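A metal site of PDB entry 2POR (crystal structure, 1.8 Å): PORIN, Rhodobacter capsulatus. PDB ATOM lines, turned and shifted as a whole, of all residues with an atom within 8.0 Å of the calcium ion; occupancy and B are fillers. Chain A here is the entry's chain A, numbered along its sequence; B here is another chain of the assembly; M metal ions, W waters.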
ATOM      1  N   LEU A 111       8.796 -29.677  16.628  1.00  0.00           N
ATOM      2  CA  LEU A 111       7.530 -29.119  16.999  1.00  0.00           C
ATOM      3  C   LEU A 111       6.459 -29.173  15.933  1.00  0.00           C
ATOM      4  O   LEU A 111       5.306 -28.798  16.161  1.00  0.00           O
ATOM      5  CB  LEU A 111       7.752 -27.685  17.415  1.00  0.00           C
ATOM      6  CG  LEU A 111       8.506 -27.477  18.705  1.00  0.00           C
ATOM      7  CD1 LEU A 111       8.782 -26.038  18.957  1.00  0.00           C
ATOM      8  CD2 LEU A 111       7.634 -27.984  19.824  1.00  0.00           C
ATOM      9  N   ALA A 113       3.474 -30.335  13.736  1.00  0.00           N
ATOM     10  CA  ALA A 113       2.379 -31.205  14.101  1.00  0.00           C
ATOM     11  C   ALA A 113       1.144 -30.827  13.301  1.00  0.00           C
ATOM     12  O   ALA A 113       1.207 -29.860  12.523  1.00  0.00           O
ATOM     13  CB  ALA A 113       2.098 -31.032  15.610  1.00  0.00           C
ATOM     14  N   GLU A 114       0.021 -31.525  13.523  1.00  0.00           N
ATOM     15  CA  GLU A 114      -1.209 -31.247  12.842  1.00  0.00           C
ATOM     16  C   GLU A 114      -1.555 -29.794  13.013  1.00  0.00           C
ATOM     17  O   GLU A 114      -1.414 -29.230  14.095  1.00  0.00           O
ATOM     18  CB  GLU A 114      -2.256 -32.154  13.428  1.00  0.00           C
ATOM     19  CG  GLU A 114      -3.609 -31.874  12.795  1.00  0.00           C
ATOM     20  CD  GLU A 114      -4.774 -32.821  13.112  1.00  0.00           C
ATOM     21  OE1 GLU A 114      -4.641 -33.665  13.987  1.00  0.00           O
ATOM     22  OE2 GLU A 114      -5.825 -32.722  12.469  1.00  0.00           O
ATOM     23  N   ASP A 115      -1.868 -29.110  11.910  1.00  0.00           N
ATOM     24  CA  ASP A 115      -2.166 -27.677  11.879  1.00  0.00           C
ATOM     25  C   ASP A 115      -1.079 -26.788  12.423  1.00  0.00           C
ATOM     26  O   ASP A 115      -1.300 -25.645  12.876  1.00  0.00           O
ATOM     27  CB  ASP A 115      -3.427 -27.350  12.672  1.00  0.00           C
ATOM     28  CG  ASP A 115      -4.704 -27.930  12.168  1.00  0.00           C
ATOM     29  OD1 ASP A 115      -4.831 -28.194  10.962  1.00  0.00           O
ATOM     30  OD2 ASP A 115      -5.602 -28.107  12.986  1.00  0.00           O
ATOM     31  N   ASN A 116       0.137 -27.303  12.376  1.00  0.00           N
ATOM     32  CA  ASN A 116       1.215 -26.546  12.964  1.00  0.00           C
ATOM     33  C   ASN A 116       2.472 -26.740  12.102  1.00  0.00           C
ATOM     34  O   ASN A 116       3.382 -27.503  12.432  1.00  0.00           O
ATOM     35  CB  ASN A 116       1.430 -27.007  14.437  1.00  0.00           C
ATOM     36  CG  ASN A 116       2.280 -25.945  15.116  1.00  0.00           C
ATOM     37  OD1 ASN A 116       1.917 -24.723  15.232  1.00  0.00           O
ATOM     38  ND2 ASN A 116       3.443 -26.420  15.595  1.00  0.00           N
ATOM     39  N   PRO A 117       2.565 -26.027  10.948  1.00  0.00           N
ATOM     40  CA  PRO A 117       3.766 -26.014  10.145  1.00  0.00           C
ATOM     41  C   PRO A 117       4.869 -25.167  10.781  1.00  0.00           C
ATOM     42  O   PRO A 117       4.572 -24.280  11.593  1.00  0.00           O
ATOM     43  CB  PRO A 117       3.252 -25.483   8.809  1.00  0.00           C
ATOM     44  CG  PRO A 117       2.187 -24.483   9.207  1.00  0.00           C
ATOM     45  CD  PRO A 117       1.496 -25.229  10.352  1.00  0.00           C
ATOM     46  N   VAL A 118       6.156 -25.388  10.445  1.00  0.00           N
ATOM     47  CA  VAL A 118       7.246 -24.497  10.851  1.00  0.00           C
ATOM     48  C   VAL A 118       7.765 -23.762   9.587  1.00  0.00           C
ATOM     49  O   VAL A 118       7.393 -24.111   8.449  1.00  0.00           O
ATOM     50  CB  VAL A 118       8.416 -25.299  11.594  1.00  0.00           C
ATOM     51  CG1 VAL A 118       7.688 -25.858  12.874  1.00  0.00           C
ATOM     52  CG2 VAL A 118       9.064 -26.497  10.865  1.00  0.00           C
ATOM     53  N   SER A 135       9.275 -21.703  14.790  1.00  0.00           N
ATOM     54  CA  SER A 135       7.923 -22.230  14.840  1.00  0.00           C
ATOM     55  C   SER A 135       7.122 -21.054  15.336  1.00  0.00           C
ATOM     56  O   SER A 135       7.689 -20.023  15.697  1.00  0.00           O
ATOM     57  CB  SER A 135       7.841 -23.435  15.796  1.00  0.00           C
ATOM     58  OG  SER A 135       8.273 -23.114  17.118  1.00  0.00           O
ATOM     59  N   ASP A 136       5.799 -21.112  15.377  1.00  0.00           N
ATOM     60  CA  ASP A 136       5.056 -19.943  15.729  1.00  0.00           C
ATOM     61  C   ASP A 136       4.720 -19.819  17.232  1.00  0.00           C
ATOM     62  O   ASP A 136       4.047 -18.842  17.575  1.00  0.00           O
ATOM     63  CB  ASP A 136       3.770 -19.929  14.900  1.00  0.00           C
ATOM     64  CG  ASP A 136       2.775 -21.052  15.092  1.00  0.00           C
ATOM     65  OD1 ASP A 136       2.698 -21.760  16.103  1.00  0.00           O
ATOM     66  OD2 ASP A 136       1.965 -21.293  14.206  1.00  0.00           O
ATOM     67  N   GLY A 137       5.045 -20.769  18.143  1.00  0.00           N
ATOM     68  CA  GLY A 137       4.770 -20.624  19.584  1.00  0.00           C
ATOM     69  C   GLY A 137       3.373 -21.007  20.035  1.00  0.00           C
ATOM     70  O   GLY A 137       3.108 -20.883  21.229  1.00  0.00           O
ATOM     71  N   LYS A 138       2.442 -21.453  19.206  1.00  0.00           N
ATOM     72  CA  LYS A 138       1.098 -21.810  19.615  1.00  0.00           C
ATOM     73  C   LYS A 138       0.752 -23.178  19.100  1.00  0.00           C
ATOM     74  O   LYS A 138       1.034 -23.508  17.932  1.00  0.00           O
ATOM     75  CB  LYS A 138       0.022 -20.890  19.086  1.00  0.00           C
ATOM     76  CG  LYS A 138       0.259 -19.446  19.455  1.00  0.00           C
ATOM     77  CD  LYS A 138       0.135 -19.343  20.934  1.00  0.00           C
ATOM     78  CE  LYS A 138       0.349 -17.953  21.423  1.00  0.00           C
ATOM     79  NZ  LYS A 138      -0.541 -17.800  22.570  1.00  0.00           N
ATOM     80  N   VAL A 139       0.130 -23.986  19.933  1.00  0.00           N
ATOM     81  CA  VAL A 139      -0.236 -25.335  19.598  1.00  0.00           C
ATOM     82  C   VAL A 139      -1.215 -25.330  18.455  1.00  0.00           C
ATOM     83  O   VAL A 139      -2.142 -24.528  18.513  1.00  0.00           O
ATOM     84  CB  VAL A 139      -0.906 -26.034  20.791  1.00  0.00           C
ATOM     85  CG1 VAL A 139      -1.301 -27.453  20.410  1.00  0.00           C
ATOM     86  CG2 VAL A 139       0.108 -26.185  21.913  1.00  0.00           C
ATOM     87  N   GLY A 140      -1.049 -26.174  17.419  1.00  0.00           N
ATOM     88  CA  GLY A 140      -1.953 -26.176  16.277  1.00  0.00           C
ATOM     89  C   GLY A 140      -2.117 -24.745  15.752  1.00  0.00           C
ATOM     90  O   GLY A 140      -1.158 -23.930  15.718  1.00  0.00           O
ATOM     91  N   GLU A 141      -3.381 -24.450  15.449  1.00  0.00           N
ATOM     92  CA  GLU A 141      -3.793 -23.105  15.064  1.00  0.00           C
ATOM     93  C   GLU A 141      -4.600 -22.538  16.219  1.00  0.00           C
ATOM     94  O   GLU A 141      -5.511 -21.731  16.004  1.00  0.00           O
ATOM     95  CB  GLU A 141      -4.650 -23.151  13.799  1.00  0.00           C
ATOM     96  CG  GLU A 141      -3.734 -23.253  12.553  1.00  0.00           C
ATOM     97  CD  GLU A 141      -4.387 -23.610  11.210  1.00  0.00           C
ATOM     98  OE1 GLU A 141      -5.605 -23.555  11.051  1.00  0.00           O
ATOM     99  OE2 GLU A 141      -3.654 -23.982  10.298  1.00  0.00           O
ATOM    100  N   THR A 142      -4.258 -22.938  17.445  1.00  0.00           N
ATOM    101  CA  THR A 142      -4.996 -22.502  18.603  1.00  0.00           C
ATOM    102  C   THR A 142      -4.270 -21.358  19.272  1.00  0.00           C
ATOM    103  O   THR A 142      -3.236 -20.881  18.793  1.00  0.00           O
ATOM    104  CB  THR A 142      -5.174 -23.675  19.643  1.00  0.00           C
ATOM    105  OG1 THR A 142      -3.938 -23.857  20.368  1.00  0.00           O
ATOM    106  CG2 THR A 142      -5.719 -24.917  18.945  1.00  0.00           C
ATOM    107  N   SER A 143      -4.781 -20.877  20.402  1.00  0.00           N
ATOM    108  CA  SER A 143      -4.071 -19.897  21.181  1.00  0.00           C
ATOM    109  C   SER A 143      -3.293 -20.526  22.332  1.00  0.00           C
ATOM    110  O   SER A 143      -2.691 -19.781  23.112  1.00  0.00           O
ATOM    111  CB  SER A 143      -5.053 -18.880  21.704  1.00  0.00           C
ATOM    112  OG  SER A 143      -5.572 -18.106  20.643  1.00  0.00           O
ATOM    113  N   GLU A 144      -3.222 -21.860  22.464  1.00  0.00           N
ATOM    114  CA  GLU A 144      -2.478 -22.437  23.572  1.00  0.00           C
ATOM    115  C   GLU A 144      -0.978 -22.293  23.380  1.00  0.00           C
ATOM    116  O   GLU A 144      -0.480 -22.641  22.306  1.00  0.00           O
ATOM    117  CB  GLU A 144      -2.900 -23.906  23.675  1.00  0.00           C
ATOM    118  CG  GLU A 144      -2.438 -24.566  24.989  1.00  0.00           C
ATOM    119  CD  GLU A 144      -2.454 -26.094  25.075  1.00  0.00           C
ATOM    120  OE1 GLU A 144      -3.247 -26.743  24.384  1.00  0.00           O
ATOM    121  OE2 GLU A 144      -1.666 -26.651  25.849  1.00  0.00           O
ATOM    122  N   ASP A 146       2.950 -22.843  23.239  1.00  0.00           N
ATOM    123  CA  ASP A 146       3.732 -24.038  22.969  1.00  0.00           C
ATOM    124  C   ASP A 146       5.158 -23.627  23.216  1.00  0.00           C
ATOM    125  O   ASP A 146       5.476 -22.455  23.445  1.00  0.00           O
ATOM    126  CB  ASP A 146       3.523 -24.476  21.467  1.00  0.00           C
ATOM    127  CG  ASP A 146       3.853 -25.925  21.120  1.00  0.00           C
ATOM    128  OD1 ASP A 146       4.394 -26.640  21.966  1.00  0.00           O
ATOM    129  OD2 ASP A 146       3.581 -26.384  20.010  1.00  0.00           O
ATOM    130  N   MET B  13      -2.607 -16.746   9.866  1.00  0.00           N
ATOM    131  CA  MET B  13      -4.036 -16.693  10.058  1.00  0.00           C
ATOM    132  C   MET B  13      -4.252 -16.232  11.520  1.00  0.00           C
ATOM    133  O   MET B  13      -3.515 -16.683  12.408  1.00  0.00           O
ATOM    134  CB  MET B  13      -4.627 -18.096   9.813  1.00  0.00           C
ATOM    135  CG  MET B  13      -6.134 -18.206  10.106  1.00  0.00           C
ATOM    136  SD  MET B  13      -6.549 -18.395  11.871  1.00  0.00           S
ATOM    137  CE  MET B  13      -5.734 -19.942  12.111  1.00  0.00           C
ATOM    138  N   TRP B  19      -2.092 -15.042  16.118  1.00  0.00           N
ATOM    139  CA  TRP B  19      -1.645 -15.376  14.775  1.00  0.00           C
ATOM    140  C   TRP B  19      -1.014 -16.770  14.810  1.00  0.00           C
ATOM    141  O   TRP B  19      -0.368 -17.121  15.809  1.00  0.00           O
ATOM    142  CB  TRP B  19      -0.597 -14.370  14.275  1.00  0.00           C
ATOM    143  CG  TRP B  19      -1.235 -13.037  13.904  1.00  0.00           C
ATOM    144  CD1 TRP B  19      -1.243 -11.994  14.775  1.00  0.00           C
ATOM    145  CD2 TRP B  19      -1.896 -12.763  12.725  1.00  0.00           C
ATOM    146  NE1 TRP B  19      -1.910 -11.039  14.155  1.00  0.00           N
ATOM    147  CE2 TRP B  19      -2.316 -11.455  12.949  1.00  0.00           C
ATOM    148  CE3 TRP B  19      -2.183 -13.408  11.538  1.00  0.00           C
ATOM    149  CZ2 TRP B  19      -3.035 -10.784  11.986  1.00  0.00           C
ATOM    150  CZ3 TRP B  19      -2.914 -12.728  10.573  1.00  0.00           C
ATOM    151  CH2 TRP B  19      -3.322 -11.429  10.799  1.00  0.00           C
ATOM    152  N   ASN B  20      -1.192 -17.584  13.771  1.00  0.00           N
ATOM    153  CA  ASN B  20      -0.505 -18.856  13.626  1.00  0.00           C
ATOM    154  C   ASN B  20      -0.087 -19.005  12.174  1.00  0.00           C
ATOM    155  O   ASN B  20      -0.775 -18.475  11.297  1.00  0.00           O
ATOM    156  CB  ASN B  20      -1.423 -20.034  13.926  1.00  0.00           C
ATOM    157  CG  ASN B  20      -1.414 -20.439  15.390  1.00  0.00           C
ATOM    158  OD1 ASN B  20      -0.534 -21.196  15.840  1.00  0.00           O
ATOM    159  ND2 ASN B  20      -2.466 -20.003  16.057  1.00  0.00           N
ATOM    160  N   PHE B  21       0.982 -19.740  11.919  1.00  0.00           N
ATOM    161  CA  PHE B  21       1.340 -20.149  10.554  1.00  0.00           C
ATOM    162  C   PHE B  21       0.274 -21.138  10.080  1.00  0.00           C
ATOM    163  O   PHE B  21      -0.207 -21.957  10.879  1.00  0.00           O
ATOM    164  CB  PHE B  21       2.717 -20.863  10.514  1.00  0.00           C
ATOM    165  CG  PHE B  21       3.964 -20.079  10.935  1.00  0.00           C
ATOM    166  CD1 PHE B  21       4.013 -18.693  10.872  1.00  0.00           C
ATOM    167  CD2 PHE B  21       5.054 -20.808  11.381  1.00  0.00           C
ATOM    168  CE1 PHE B  21       5.160 -18.068  11.271  1.00  0.00           C
ATOM    169  CE2 PHE B  21       6.202 -20.150  11.766  1.00  0.00           C
ATOM    170  CZ  PHE B  21       6.248 -18.787  11.718  1.00  0.00           C
ATOM    171  N   SER B  22      -0.168 -21.110   8.819  1.00  0.00           N
ATOM    172  CA  SER B  22      -1.166 -22.030   8.307  1.00  0.00           C
ATOM    173  C   SER B  22      -0.781 -22.360   6.860  1.00  0.00           C
ATOM    174  O   SER B  22      -0.634 -21.444   6.044  1.00  0.00           O
ATOM    175  CB  SER B  22      -2.507 -21.394   8.362  1.00  0.00           C
ATOM    176  OG  SER B  22      -3.485 -22.354   8.061  1.00  0.00           O
HETATM  177 CA    CA M   1       0.754 -22.921  15.462  1.00  0.00          CA
HETATM  178  O   HOH W   1       0.030 -23.363  13.278  1.00  0.00           O
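The side-chain amide nitrogen (ND2) of Asn 116 is in hydrogen-bond range of the backbone carbonyl oxygen (O) of Leu 111 (3.1 Å). The backbone carbonyl oxygen (O) of Thr 142 lies within hydrogen-bond range of the side-chain amide nitrogen (ND2) of Asn 20 of chain B, 3.0 Å away. N of Asn 20 of chain B sits at hydrogen-bond distance from O of Met 13 of chain B. The side-chain carboxylate of Asp 136 lies close to the backbone NH of Phe 21 of chain B, at 2.9 Å. NZ of Lys 138 lies within hydrogen-bond range of O of Ser 143, 3.0 Å away.
Five residues have an atom within 4 Å of the calcium ion: Asn 116, Asp 136, Lys 138, Gly 140 and Asn 20 of chain B.
The calcium ion is bound by the side-chain amide oxygen (OD1) of Asn 116 (2.2 Å), the backbone carbonyl oxygen (O) of Gly 140 (2.2 Å), the side-chain amide oxygen (OD1) of Asn 20 of chain B (2.2 Å), water W1 (2.3 Å), the side-chain carboxylate (OD1) of Asp 136 (2.4 Å), the side-chain carboxylate (OD2) of Asp 136 (2.4 Å) and the backbone carbonyl oxygen (O) of Lys 138 (2.6 Å).
Water W1 bridges the backbone carbonyl oxygen of Asp 115 and the backbone carbonyl oxygen of Phe 21 of chain B.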
